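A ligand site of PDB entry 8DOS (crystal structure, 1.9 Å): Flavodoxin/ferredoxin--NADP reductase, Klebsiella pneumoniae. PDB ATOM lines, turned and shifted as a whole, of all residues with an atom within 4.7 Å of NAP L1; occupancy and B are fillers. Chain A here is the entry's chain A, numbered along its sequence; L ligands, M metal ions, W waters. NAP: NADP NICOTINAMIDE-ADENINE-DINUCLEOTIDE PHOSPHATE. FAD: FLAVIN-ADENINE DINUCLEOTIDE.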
ATOM      1  N   ALA A  26     -15.468  27.331 -14.596  1.00  0.00           N
ATOM      2  CA  ALA A  26     -16.388  26.318 -15.081  1.00  0.00           C
ATOM      3  C   ALA A  26     -17.564  26.053 -14.154  1.00  0.00           C
ATOM      4  O   ALA A  26     -18.586  25.528 -14.619  1.00  0.00           O
ATOM      5  CB  ALA A  26     -15.649  24.993 -15.332  1.00  0.00           C
ATOM      6  N   LEU A  27     -17.468  26.424 -12.878  1.00  0.00           N
ATOM      7  CA  LEU A  27     -18.503  26.156 -11.885  1.00  0.00           C
ATOM      8  C   LEU A  27     -19.310  27.424 -11.615  1.00  0.00           C
ATOM      9  O   LEU A  27     -18.724  28.500 -11.459  1.00  0.00           O
ATOM     10  CB  LEU A  27     -17.862  25.670 -10.586  1.00  0.00           C
ATOM     11  CG  LEU A  27     -17.156  24.333 -10.747  1.00  0.00           C
ATOM     12  CD1 LEU A  27     -16.252  24.035  -9.560  1.00  0.00           C
ATOM     13  CD2 LEU A  27     -18.211  23.231 -10.916  1.00  0.00           C
ATOM     14  N   VAL A  76     -21.878  22.717 -13.600  1.00  0.00           N
ATOM     15  CA  VAL A  76     -20.561  22.759 -14.205  1.00  0.00           C
ATOM     16  C   VAL A  76     -20.749  22.883 -15.706  1.00  0.00           C
ATOM     17  O   VAL A  76     -21.646  22.252 -16.284  1.00  0.00           O
ATOM     18  CB  VAL A  76     -19.710  21.528 -13.819  1.00  0.00           C
ATOM     19  CG1 VAL A  76     -20.342  20.249 -14.349  1.00  0.00           C
ATOM     20  CG2 VAL A  76     -18.277  21.692 -14.296  1.00  0.00           C
ATOM     21  N   THR A  77     -19.954  23.762 -16.329  1.00  0.00           N
ATOM     22  CA  THR A  77     -19.981  23.861 -17.784  1.00  0.00           C
ATOM     23  C   THR A  77     -19.301  22.633 -18.361  1.00  0.00           C
ATOM     24  O   THR A  77     -18.099  22.416 -18.151  1.00  0.00           O
ATOM     25  CB  THR A  77     -19.264  25.115 -18.289  1.00  0.00           C
ATOM     26  OG1 THR A  77     -19.855  26.275 -17.696  1.00  0.00           O
ATOM     27  CG2 THR A  77     -19.471  25.216 -19.793  1.00  0.00           C
ATOM     28  N   PRO A  79     -17.676  20.991 -21.357  1.00  0.00           N
ATOM     29  CA  PRO A  79     -17.044  21.626 -22.531  1.00  0.00           C
ATOM     30  C   PRO A  79     -17.822  21.491 -23.837  1.00  0.00           C
ATOM     31  O   PRO A  79     -18.180  22.513 -24.451  1.00  0.00           O
ATOM     32  CB  PRO A  79     -15.700  20.898 -22.614  1.00  0.00           C
ATOM     33  CG  PRO A  79     -15.412  20.453 -21.226  1.00  0.00           C
ATOM     34  CD  PRO A  79     -16.737  20.182 -20.572  1.00  0.00           C
ATOM     35  N   THR A 122     -20.043  14.099  -5.342  1.00  0.00           N
ATOM     36  CA  THR A 122     -18.931  14.594  -6.152  1.00  0.00           C
ATOM     37  C   THR A 122     -19.371  15.867  -6.855  1.00  0.00           C
ATOM     38  O   THR A 122     -20.530  15.995  -7.264  1.00  0.00           O
ATOM     39  CB  THR A 122     -18.494  13.600  -7.253  1.00  0.00           C
ATOM     40  OG1 THR A 122     -19.563  13.422  -8.184  1.00  0.00           O
ATOM     41  CG2 THR A 122     -18.068  12.246  -6.662  1.00  0.00           C
ATOM     42  N   GLY A 123     -18.435  16.796  -7.020  1.00  0.00           N
ATOM     43  CA  GLY A 123     -18.626  17.894  -7.966  1.00  0.00           C
ATOM     44  C   GLY A 123     -19.887  18.686  -7.688  1.00  0.00           C
ATOM     45  O   GLY A 123     -20.114  19.152  -6.571  1.00  0.00           O
ATOM     46  N   THR A 124     -20.731  18.852  -8.704  1.00  0.00           N
ATOM     47  CA  THR A 124     -21.928  19.668  -8.538  1.00  0.00           C
ATOM     48  C   THR A 124     -23.105  18.872  -8.002  1.00  0.00           C
ATOM     49  O   THR A 124     -24.230  19.384  -8.014  1.00  0.00           O
ATOM     50  CB  THR A 124     -22.305  20.353  -9.854  1.00  0.00           C
ATOM     51  OG1 THR A 124     -22.531  19.373 -10.877  1.00  0.00           O
ATOM     52  CG2 THR A 124     -21.202  21.280 -10.302  1.00  0.00           C
ATOM     53  N   ALA A 150     -16.548  15.753  -2.650  1.00  0.00           N
ATOM     54  CA  ALA A 150     -15.331  15.300  -3.306  1.00  0.00           C
ATOM     55  C   ALA A 150     -15.207  16.027  -4.645  1.00  0.00           C
ATOM     56  O   ALA A 150     -16.145  16.036  -5.446  1.00  0.00           O
ATOM     57  CB  ALA A 150     -15.361  13.776  -3.518  1.00  0.00           C
ATOM     58  N   VAL A 151     -14.050  16.657  -4.872  1.00  0.00           N
ATOM     59  CA  VAL A 151     -13.811  17.477  -6.062  1.00  0.00           C
ATOM     60  C   VAL A 151     -12.364  17.274  -6.511  1.00  0.00           C
ATOM     61  O   VAL A 151     -11.549  16.684  -5.800  1.00  0.00           O
ATOM     62  CB  VAL A 151     -14.065  18.968  -5.794  1.00  0.00           C
ATOM     63  CG1 VAL A 151     -15.523  19.210  -5.340  1.00  0.00           C
ATOM     64  CG2 VAL A 151     -13.085  19.473  -4.732  1.00  0.00           C
ATOM     65  N   ARG A 152     -12.046  17.813  -7.683  1.00  0.00           N
ATOM     66  CA  ARG A 152     -10.673  17.697  -8.171  1.00  0.00           C
ATOM     67  C   ARG A 152      -9.722  18.639  -7.452  1.00  0.00           C
ATOM     68  O   ARG A 152      -8.603  18.250  -7.105  1.00  0.00           O
ATOM     69  CB  ARG A 152     -10.611  17.991  -9.670  1.00  0.00           C
ATOM     70  CG  ARG A 152     -11.479  17.101 -10.513  1.00  0.00           C
ATOM     71  CD  ARG A 152     -11.235  17.397 -11.978  1.00  0.00           C
ATOM     72  NE  ARG A 152     -12.168  16.665 -12.812  1.00  0.00           N
ATOM     73  CZ  ARG A 152     -11.963  16.388 -14.092  1.00  0.00           C
ATOM     74  NH1 ARG A 152     -10.882  16.790 -14.727  1.00  0.00           N
ATOM     75  NH2 ARG A 152     -12.871  15.665 -14.748  1.00  0.00           N
ATOM     76  N   TYR A 153     -10.139  19.884  -7.246  1.00  0.00           N
ATOM     77  CA  TYR A 153      -9.249  20.908  -6.708  1.00  0.00           C
ATOM     78  C   TYR A 153      -9.954  21.671  -5.594  1.00  0.00           C
ATOM     79  O   TYR A 153     -11.175  21.811  -5.607  1.00  0.00           O
ATOM     80  CB  TYR A 153      -8.796  21.891  -7.790  1.00  0.00           C
ATOM     81  CG  TYR A 153      -7.867  21.256  -8.786  1.00  0.00           C
ATOM     82  CD1 TYR A 153      -6.529  21.074  -8.496  1.00  0.00           C
ATOM     83  CD2 TYR A 153      -8.336  20.821 -10.018  1.00  0.00           C
ATOM     84  CE1 TYR A 153      -5.659  20.479  -9.409  1.00  0.00           C
ATOM     85  CE2 TYR A 153      -7.470  20.218 -10.941  1.00  0.00           C
ATOM     86  CZ  TYR A 153      -6.145  20.057 -10.624  1.00  0.00           C
ATOM     87  OH  TYR A 153      -5.289  19.470 -11.535  1.00  0.00           O
ATOM     88  N   ASP A 156     -12.578  24.185  -6.211  1.00  0.00           N
ATOM     89  CA  ASP A 156     -13.886  23.687  -6.645  1.00  0.00           C
ATOM     90  C   ASP A 156     -14.885  23.512  -5.504  1.00  0.00           C
ATOM     91  O   ASP A 156     -16.016  23.084  -5.753  1.00  0.00           O
ATOM     92  CB  ASP A 156     -13.733  22.344  -7.377  1.00  0.00           C
ATOM     93  CG  ASP A 156     -12.851  22.437  -8.610  1.00  0.00           C
ATOM     94  OD1 ASP A 156     -12.652  23.545  -9.167  1.00  0.00           O
ATOM     95  OD2 ASP A 156     -12.337  21.380  -9.027  1.00  0.00           O
ATOM     96  N   SER A 181      -9.060  15.491  -4.997  1.00  0.00           N
ATOM     97  CA  SER A 181      -8.409  14.336  -5.612  1.00  0.00           C
ATOM     98  C   SER A 181      -7.106  14.650  -6.344  1.00  0.00           C
ATOM     99  O   SER A 181      -6.283  13.749  -6.495  1.00  0.00           O
ATOM    100  CB  SER A 181      -9.361  13.625  -6.583  1.00  0.00           C
ATOM    101  OG  SER A 181      -9.960  14.557  -7.479  1.00  0.00           O
ATOM    102  N   ARG A 182      -6.890  15.895  -6.792  1.00  0.00           N
ATOM    103  CA  ARG A 182      -5.760  16.189  -7.662  1.00  0.00           C
ATOM    104  C   ARG A 182      -4.715  17.096  -7.027  1.00  0.00           C
ATOM    105  O   ARG A 182      -3.743  17.469  -7.683  1.00  0.00           O
ATOM    106  CB  ARG A 182      -6.246  16.803  -8.968  1.00  0.00           C
ATOM    107  CG  ARG A 182      -7.486  16.107  -9.514  1.00  0.00           C
ATOM    108  CD  ARG A 182      -7.560  16.148 -11.009  1.00  0.00           C
ATOM    109  NE  ARG A 182      -8.465  15.146 -11.556  1.00  0.00           N
ATOM    110  CZ  ARG A 182      -8.584  14.905 -12.850  1.00  0.00           C
ATOM    111  NH1 ARG A 182      -7.853  15.548 -13.749  1.00  0.00           N
ATOM    112  NH2 ARG A 182      -9.449  13.983 -13.269  1.00  0.00           N
ATOM    113  N   ARG A 192      -9.678   9.633  -3.752  1.00  0.00           N
ATOM    114  CA  ARG A 192     -11.020   9.267  -4.183  1.00  0.00           C
ATOM    115  C   ARG A 192     -11.734   8.561  -3.049  1.00  0.00           C
ATOM    116  O   ARG A 192     -11.121   7.897  -2.226  1.00  0.00           O
ATOM    117  CB  ARG A 192     -10.975   8.369  -5.413  1.00  0.00           C
ATOM    118  CG  ARG A 192     -10.600   9.104  -6.707  1.00  0.00           C
ATOM    119  CD  ARG A 192     -10.407   8.108  -7.804  1.00  0.00           C
ATOM    120  NE  ARG A 192     -10.475   8.720  -9.127  1.00  0.00           N
ATOM    121  CZ  ARG A 192     -10.747   8.046 -10.232  1.00  0.00           C
ATOM    122  NH1 ARG A 192     -10.911   6.729 -10.223  1.00  0.00           N
ATOM    123  NH2 ARG A 192     -10.850   8.714 -11.382  1.00  0.00           N
ATOM    124  N   VAL A 193     -13.061   8.707  -3.027  1.00  0.00           N
ATOM    125  CA  VAL A 193     -13.826   8.233  -1.880  1.00  0.00           C
ATOM    126  C   VAL A 193     -13.660   6.727  -1.645  1.00  0.00           C
ATOM    127  O   VAL A 193     -13.466   6.337  -0.496  1.00  0.00           O
ATOM    128  CB  VAL A 193     -15.288   8.685  -2.008  1.00  0.00           C
ATOM    129  CG1 VAL A 193     -16.182   7.932  -0.999  1.00  0.00           C
ATOM    130  CG2 VAL A 193     -15.347  10.199  -1.764  1.00  0.00           C
ATOM    131  N   PRO A 194     -13.719   5.849  -2.653  1.00  0.00           N
ATOM    132  CA  PRO A 194     -13.542   4.412  -2.334  1.00  0.00           C
ATOM    133  C   PRO A 194     -12.198   4.107  -1.695  1.00  0.00           C
ATOM    134  O   PRO A 194     -12.119   3.280  -0.782  1.00  0.00           O
ATOM    135  CB  PRO A 194     -13.720   3.717  -3.691  1.00  0.00           C
ATOM    136  CG  PRO A 194     -14.555   4.686  -4.501  1.00  0.00           C
ATOM    137  CD  PRO A 194     -14.105   6.055  -4.065  1.00  0.00           C
ATOM    138  N   ASN A 222     -21.052  11.646  -9.782  1.00  0.00           N
ATOM    139  CA  ASN A 222     -20.279  10.976 -10.829  1.00  0.00           C
ATOM    140  C   ASN A 222     -20.648   9.501 -10.842  1.00  0.00           C
ATOM    141  O   ASN A 222     -20.490   8.818  -9.818  1.00  0.00           O
ATOM    142  CB  ASN A 222     -18.782  11.180 -10.587  1.00  0.00           C
ATOM    143  CG  ASN A 222     -17.927  10.545 -11.679  1.00  0.00           C
ATOM    144  OD1 ASN A 222     -17.933   9.327 -11.845  1.00  0.00           O
ATOM    145  ND2 ASN A 222     -17.189  11.363 -12.428  1.00  0.00           N
ATOM    146  N   GLN A 224     -19.356   6.820 -12.079  1.00  0.00           N
ATOM    147  CA  GLN A 224     -18.298   5.854 -11.807  1.00  0.00           C
ATOM    148  C   GLN A 224     -17.999   5.792 -10.319  1.00  0.00           C
ATOM    149  O   GLN A 224     -17.763   4.713  -9.774  1.00  0.00           O
ATOM    150  CB  GLN A 224     -17.039   6.226 -12.569  1.00  0.00           C
ATOM    151  CG  GLN A 224     -17.219   6.265 -14.068  1.00  0.00           C
ATOM    152  CD  GLN A 224     -16.838   7.632 -14.600  1.00  0.00           C
ATOM    153  OE1 GLN A 224     -15.751   8.153 -14.294  1.00  0.00           O
ATOM    154  NE2 GLN A 224     -17.739   8.230 -15.370  1.00  0.00           N
ATOM    155  N   MET A 225     -17.981   6.952  -9.676  1.00  0.00           N
ATOM    156  CA  MET A 225     -17.764   6.988  -8.231  1.00  0.00           C
ATOM    157  C   MET A 225     -18.895   6.274  -7.504  1.00  0.00           C
ATOM    158  O   MET A 225     -18.640   5.515  -6.563  1.00  0.00           O
ATOM    159  CB  MET A 225     -17.609   8.456  -7.792  1.00  0.00           C
ATOM    160  CG  MET A 225     -17.761   8.791  -6.307  1.00  0.00           C
ATOM    161  SD  MET A 225     -19.333   8.580  -5.448  1.00  0.00           S
ATOM    162  CE  MET A 225     -18.791   8.994  -3.795  1.00  0.00           C
ATOM    163  N   ARG A 227     -20.821   3.897  -8.767  1.00  0.00           N
ATOM    164  CA  ARG A 227     -20.614   2.483  -9.059  1.00  0.00           C
ATOM    165  C   ARG A 227     -19.464   1.899  -8.228  1.00  0.00           C
ATOM    166  O   ARG A 227     -19.639   0.879  -7.541  1.00  0.00           O
ATOM    167  CB  ARG A 227     -20.347   2.328 -10.561  1.00  0.00           C
ATOM    168  CG  ARG A 227     -19.789   0.975 -10.998  1.00  0.00           C
ATOM    169  CD  ARG A 227     -19.029   1.136 -12.327  1.00  0.00           C
ATOM    170  NE  ARG A 227     -17.694   1.734 -12.156  1.00  0.00           N
ATOM    171  CZ  ARG A 227     -16.942   2.199 -13.150  1.00  0.00           C
ATOM    172  NH1 ARG A 227     -17.356   2.160 -14.407  1.00  0.00           N
ATOM    173  NH2 ARG A 227     -15.744   2.708 -12.859  1.00  0.00           N
ATOM    174  N   ASP A 228     -18.300   2.550  -8.260  1.00  0.00           N
ATOM    175  CA  ASP A 228     -17.130   1.978  -7.587  1.00  0.00           C
ATOM    176  C   ASP A 228     -17.284   1.987  -6.078  1.00  0.00           C
ATOM    177  O   ASP A 228     -16.815   1.066  -5.402  1.00  0.00           O
ATOM    178  CB  ASP A 228     -15.871   2.739  -8.015  1.00  0.00           C
ATOM    179  CG  ASP A 228     -15.502   2.471  -9.455  1.00  0.00           C
ATOM    180  OD1 ASP A 228     -16.132   1.570 -10.036  1.00  0.00           O
ATOM    181  OD2 ASP A 228     -14.618   3.190 -10.004  1.00  0.00           O
ATOM    182  N   TRP A 256     -25.117  11.110 -14.549  1.00  0.00           N
ATOM    183  CA  TRP A 256     -25.220  10.706 -15.957  1.00  0.00           C
ATOM    184  C   TRP A 256     -25.009   9.206 -16.113  1.00  0.00           C
ATOM    185  O   TRP A 256     -24.799   8.462 -15.172  1.00  0.00           O
ATOM    186  CB  TRP A 256     -24.250  11.490 -16.865  1.00  0.00           C
ATOM    187  CG  TRP A 256     -22.768  11.361 -16.617  1.00  0.00           C
ATOM    188  CD1 TRP A 256     -21.859  10.629 -17.354  1.00  0.00           C
ATOM    189  CD2 TRP A 256     -22.004  12.048 -15.614  1.00  0.00           C
ATOM    190  NE1 TRP A 256     -20.588  10.790 -16.844  1.00  0.00           N
ATOM    191  CE2 TRP A 256     -20.651  11.668 -15.787  1.00  0.00           C
ATOM    192  CE3 TRP A 256     -22.336  12.944 -14.595  1.00  0.00           C
ATOM    193  CZ2 TRP A 256     -19.624  12.148 -14.954  1.00  0.00           C
ATOM    194  CZ3 TRP A 256     -21.316  13.421 -13.756  1.00  0.00           C
ATOM    195  CH2 TRP A 256     -19.987  13.011 -13.942  1.00  0.00           C
ATOM    196  OXT TRP A 256     -25.095   8.681 -17.207  1.00  0.00           O
HETATM  197  PA  NAP L   1     -15.874  14.830 -11.963  1.00  0.00           P
HETATM  198  O1A NAP L   1     -14.998  14.602 -13.156  1.00  0.00           O
HETATM  199  O2A NAP L   1     -17.097  13.992 -11.805  1.00  0.00           O
HETATM  200  O5B NAP L   1     -14.948  14.676 -10.657  1.00  0.00           O
HETATM  201  C5B NAP L   1     -15.483  14.870  -9.319  1.00  0.00           C
HETATM  202  C4B NAP L   1     -14.714  13.980  -8.385  1.00  0.00           C
HETATM  203  O4B NAP L   1     -15.071  12.603  -8.664  1.00  0.00           O
HETATM  204  C3B NAP L   1     -13.176  14.034  -8.512  1.00  0.00           C
HETATM  205  O3B NAP L   1     -12.615  14.133  -7.219  1.00  0.00           O
HETATM  206  C2B NAP L   1     -12.829  12.684  -9.143  1.00  0.00           C
HETATM  207  O2B NAP L   1     -11.560  12.145  -8.794  1.00  0.00           O
HETATM  208  C1B NAP L   1     -13.910  11.822  -8.528  1.00  0.00           C
HETATM  209  N9A NAP L   1     -14.088  10.559  -9.245  1.00  0.00           N
HETATM  210  C8A NAP L   1     -14.106  10.405 -10.605  1.00  0.00           C
HETATM  211  N7A NAP L   1     -14.245   9.167 -10.994  1.00  0.00           N
HETATM  212  C5A NAP L   1     -14.285   8.446  -9.801  1.00  0.00           C
HETATM  213  C6A NAP L   1     -14.415   7.069  -9.531  1.00  0.00           C
HETATM  214  N6A NAP L   1     -14.491   6.139 -10.484  1.00  0.00           N
HETATM  215  N1A NAP L   1     -14.413   6.681  -8.237  1.00  0.00           N
HETATM  216  C2A NAP L   1     -14.317   7.624  -7.285  1.00  0.00           C
HETATM  217  N3A NAP L   1     -14.207   8.943  -7.419  1.00  0.00           N
HETATM  218  C4A NAP L   1     -14.192   9.304  -8.721  1.00  0.00           C
HETATM  219  O3  NAP L   1     -16.409  16.340 -11.905  1.00  0.00           O
HETATM  220  PN  NAP L   1     -16.033  17.896 -12.104  1.00  0.00           P
HETATM  221  O1N NAP L   1     -14.627  18.131 -11.636  1.00  0.00           O
HETATM  222  O2N NAP L   1     -17.108  18.711 -11.461  1.00  0.00           O
HETATM  223  O5D NAP L   1     -16.154  18.129 -13.688  1.00  0.00           O
HETATM  224  C5D NAP L   1     -15.097  17.770 -14.599  1.00  0.00           C
HETATM  225  C4D NAP L   1     -15.428  18.325 -15.954  1.00  0.00           C
HETATM  226  O4D NAP L   1     -15.672  19.742 -15.815  1.00  0.00           O
HETATM  227  C3D NAP L   1     -14.295  18.258 -16.983  1.00  0.00           C
HETATM  228  O3D NAP L   1     -14.816  18.527 -18.282  1.00  0.00           O
HETATM  229  C2D NAP L   1     -13.434  19.428 -16.481  1.00  0.00           C
HETATM  230  O2D NAP L   1     -12.542  19.964 -17.443  1.00  0.00           O
HETATM  231  C1D NAP L   1     -14.446  20.455 -15.977  1.00  0.00           C
HETATM  232  N1N NAP L   1     -14.021  20.991 -14.648  1.00  0.00           N
HETATM  233  C2N NAP L   1     -12.710  21.304 -14.426  1.00  0.00           C
HETATM  234  C3N NAP L   1     -12.261  21.536 -13.130  1.00  0.00           C
HETATM  235  C7N NAP L   1     -10.782  21.721 -12.904  1.00  0.00           C
HETATM  236  O7N NAP L   1     -10.147  20.855 -12.328  1.00  0.00           O
HETATM  237  N7N NAP L   1     -10.235  22.850 -13.349  1.00  0.00           N
HETATM  238  C4N NAP L   1     -13.187  21.571 -12.082  1.00  0.00           C
HETATM  239  C5N NAP L   1     -14.535  21.452 -12.362  1.00  0.00           C
HETATM  240  C6N NAP L   1     -14.930  21.161 -13.650  1.00  0.00           C
HETATM  241  P2B NAP L   1     -10.372  12.255  -9.922  1.00  0.00           P
HETATM  242  O1X NAP L   1      -9.430  11.131  -9.536  1.00  0.00           O
HETATM  243  O2X NAP L   1     -10.979  12.058 -11.291  1.00  0.00           O
HETATM  244  O3X NAP L   1      -9.750  13.626  -9.745  1.00  0.00           O
HETATM  245  PA  FAD L   2     -24.535  16.484 -22.571  1.00  0.00           P
HETATM  246  O1A FAD L   2     -25.963  16.147 -22.700  1.00  0.00           O
HETATM  247  O2A FAD L   2     -23.865  16.772 -23.903  1.00  0.00           O
HETATM  248  O5B FAD L   2     -23.860  15.384 -21.552  1.00  0.00           O
HETATM  249  C5B FAD L   2     -22.602  14.750 -21.859  1.00  0.00           C
HETATM  250  C4B FAD L   2     -21.662  14.568 -20.689  1.00  0.00           C
HETATM  251  O4B FAD L   2     -21.722  15.635 -19.726  1.00  0.00           O
HETATM  252  C3B FAD L   2     -21.884  13.358 -19.794  1.00  0.00           C
HETATM  253  O3B FAD L   2     -21.649  12.137 -20.475  1.00  0.00           O
HETATM  254  C2B FAD L   2     -20.894  13.657 -18.681  1.00  0.00           C
HETATM  255  O2B FAD L   2     -19.570  13.396 -19.133  1.00  0.00           O
HETATM  256  C1B FAD L   2     -21.023  15.180 -18.561  1.00  0.00           C
HETATM  257  N9A FAD L   2     -21.724  15.610 -17.364  1.00  0.00           N
HETATM  258  C8A FAD L   2     -23.077  15.672 -17.193  1.00  0.00           C
HETATM  259  N7A FAD L   2     -23.448  16.120 -16.015  1.00  0.00           N
HETATM  260  C5A FAD L   2     -22.252  16.342 -15.363  1.00  0.00           C
HETATM  261  C6A FAD L   2     -21.946  16.796 -14.059  1.00  0.00           C
HETATM  262  N6A FAD L   2     -22.878  17.144 -13.162  1.00  0.00           N
HETATM  263  N1A FAD L   2     -20.647  16.898 -13.716  1.00  0.00           N
HETATM  264  C2A FAD L   2     -19.716  16.559 -14.610  1.00  0.00           C
HETATM  265  N3A FAD L   2     -19.881  16.116 -15.858  1.00  0.00           N
HETATM  266  C4A FAD L   2     -21.176  16.027 -16.175  1.00  0.00           C
HETATM  267  N1  FAD L   2     -25.724  18.638 -13.436  1.00  0.00           N
HETATM  268  C2  FAD L   2     -25.317  19.747 -12.770  1.00  0.00           C
HETATM  269  O2  FAD L   2     -24.392  20.449 -13.185  1.00  0.00           O
HETATM  270  N3  FAD L   2     -25.966  20.119 -11.602  1.00  0.00           N
HETATM  271  C4  FAD L   2     -27.005  19.435 -10.997  1.00  0.00           C
HETATM  272  O4  FAD L   2     -27.511  19.845  -9.952  1.00  0.00           O
HETATM  273  C4X FAD L   2     -27.426  18.257 -11.718  1.00  0.00           C
HETATM  274  N5  FAD L   2     -28.392  17.554 -11.218  1.00  0.00           N
HETATM  275  C5X FAD L   2     -28.791  16.434 -11.879  1.00  0.00           C
HETATM  276  C6  FAD L   2     -29.822  15.662 -11.326  1.00  0.00           C
HETATM  277  C7  FAD L   2     -30.271  14.508 -11.967  1.00  0.00           C
HETATM  278  C7M FAD L   2     -31.386  13.705 -11.351  1.00  0.00           C
HETATM  279  C8  FAD L   2     -29.665  14.110 -13.171  1.00  0.00           C
HETATM  280  C8M FAD L   2     -30.124  12.863 -13.889  1.00  0.00           C
HETATM  281  C9  FAD L   2     -28.640  14.869 -13.721  1.00  0.00           C
HETATM  282  C9A FAD L   2     -28.191  16.024 -13.080  1.00  0.00           C
HETATM  283  N10 FAD L   2     -27.117  16.793 -13.577  1.00  0.00           N
HETATM  284  C10 FAD L   2     -26.726  17.938 -12.930  1.00  0.00           C
HETATM  285  C1' FAD L   2     -26.541  16.529 -14.911  1.00  0.00           C
HETATM  286  C2' FAD L   2     -27.316  17.341 -15.963  1.00  0.00           C
HETATM  287  O2' FAD L   2     -28.666  16.870 -16.107  1.00  0.00           O
HETATM  288  C3' FAD L   2     -26.611  17.354 -17.318  1.00  0.00           C
HETATM  289  O3' FAD L   2     -26.283  16.043 -17.780  1.00  0.00           O
HETATM  290  C4' FAD L   2     -25.414  18.308 -17.416  1.00  0.00           C
HETATM  291  O4' FAD L   2     -25.846  19.632 -17.103  1.00  0.00           O
HETATM  292  C5' FAD L   2     -24.728  18.275 -18.766  1.00  0.00           C
HETATM  293  O5' FAD L   2     -25.692  18.538 -19.806  1.00  0.00           O
HETATM  294  P   FAD L   2     -25.224  19.015 -21.246  1.00  0.00           P
HETATM  295  O1P FAD L   2     -26.393  19.147 -22.225  1.00  0.00           O
HETATM  296  O2P FAD L   2     -24.365  20.176 -21.047  1.00  0.00           O
HETATM  297  O3P FAD L   2     -24.340  17.777 -21.677  1.00  0.00           O
HETATM  298 CA    CA M   1     -14.358  11.673 -16.406  1.00  0.00          CA
HETATM  299  O   HOH W   1     -14.011  19.078  -9.180  1.00  0.00           O
HETATM  300  O   HOH W   2     -19.055  14.931 -10.275  1.00  0.00           O
HETATM  301  O   HOH W   3      -9.074  19.322 -14.122  1.00  0.00           O
HETATM  302  O   HOH W   4     -19.656  17.557 -11.197  1.00  0.00           O
HETATM  303  O   HOH W   5      -7.120  11.176  -8.212  1.00  0.00           O
HETATM  304  O   HOH W   6     -10.325  24.474 -10.295  1.00  0.00           O
HETATM  305  O   HOH W   7     -16.349  20.110  -9.459  1.00  0.00           O
HETATM  306  O   HOH W   8     -13.738   6.434 -13.434  1.00  0.00           O
HETATM  307  O   HOH W   9     -12.565   4.468  -7.426  1.00  0.00           O
HETATM  308  O   HOH W  10     -14.283  10.239  -4.947  1.00  0.00           O
HETATM  309  O   HOH W  11     -12.532  12.615  -5.091  1.00  0.00           O
HETATM  310  O   HOH W  12     -13.706  24.517 -11.544  1.00  0.00           O
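Water W3 bridges an oxygen (O7N) of NAP L1 and the guanidinium group of Arg 152. Water W5 lies within hydrogen-bond range of an oxygen (O1X) of NAP L1 (2.7 Å) and the backbone carbonyl oxygen (O) of Ser 181 (3.2 Å). Water W10 lies within hydrogen-bond range of N of Val 193 (2.7 Å) and N3A of NAP L1 (2.8 Å). Water W4 lies within hydrogen-bond range of a nitrogen (N1A) of FAD L2 (2.8 Å), an oxygen (O2N) of NAP L1 (2.8 Å) and the backbone NH (N) of Thr 124 (3.0 Å). Water W8 bridges OE1 of Gln 224 and N6A of NAP L1. Water W6 lies within hydrogen-bond range of the side-chain carboxylate of Asp 156 and a nitrogen (N7N) of NAP L1.
The backbone NH (N) of Arg 182 is in hydrogen-bond range of the backbone carbonyl oxygen (O) of Arg 152, 2.9 Å away. The side-chain amide oxygen of Asn 222 sits at hydrogen-bond distance from the backbone NH of Met 225. OD2 of Asp 156 lies within hydrogen-bond range of N of Tyr 153 (3.2 Å). N of Gln 224 is in hydrogen-bond range of OD1 of Asn 222, 2.9 Å away. O of Ala 150 is in hydrogen-bond range of N of Gly 123, 2.9 Å away. The side-chain carboxylate of Asp 228 is in salt-bridge range of the guanidinium group of Arg 227, 2.6 Å away. N of Asn 222 lies within hydrogen-bond range of OG1 of Thr 122. N of Ser 181 is in hydrogen-bond range of O of Val 151 (2.9 Å).
The side-chain hydroxyl (OG) of Ser 181 sits at hydrogen-bond distance from an oxygen (O3X) of NAP L1, 2.5 Å away. The backbone NH (N) of Val 76 is in hydrogen-bond range of an oxygen (O2) of FAD L2 (3.4 Å). An oxygen (O1X) of NAP L1 is in salt-bridge range of the guanidinium group (NE) of Arg 192 (2.7 Å). The side-chain hydroxyl of Thr 124 sits at hydrogen-bond distance from an oxygen (O2) of FAD L2 (3.2 Å). O2A of NAP L1 is in hydrogen-bond range of ND2 of Asn 222 (2.7 Å). O1A of NAP L1 is in salt-bridge range of NH2 of Arg 152 (2.9 Å). OD2 of Asp 228 is in hydrogen-bond range of N6A of NAP L1 (3.0 Å). NE of Arg 182 lies within salt-bridge range of O3X of NAP L1, 2.7 Å away. An oxygen (O3B) of NAP L1 lies within hydrogen-bond range of the backbone carbonyl oxygen (O) of Val 151 (3.1 Å).
Val 76 touches NAP L1 (CG2 to C6N, 3.4 Å). Pro 79 touches NAP L1 (CD to O3D, 3.4 Å). CG2 of Thr 122 touches O4B of NAP L1 (3.6 Å). Gly 123 touches NAP L1. Ala 150 touches NAP L1. Tyr 153 touches NAP L1 (CD2 to O7N, 2.9 Å). OD2 of Asp 156 touches C4N of NAP L1, 3.2 Å away. CD of Pro 194 touches C2A of NAP L1 (3.6 Å). Gln 224 touches NAP L1 (CB to N6A, 3.3 Å). CA of Met 225 touches N1A of NAP L1, 3.4 Å away. Trp 256 touches NAP L1. 18 residues have an atom within 4 Å of NAP L1: Val 76, Pro 79, Thr 122, Gly 123, Ala 150, Val 151, Arg 152, Tyr 153, Asp 156, Ser 181, Arg 182, Arg 192, Pro 194, Asn 222, Gln 224, Met 225, Asp 228 and Trp 256. The nearest printed residue that does not touch NAP L1 is Leu 27 (4.2 Å).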
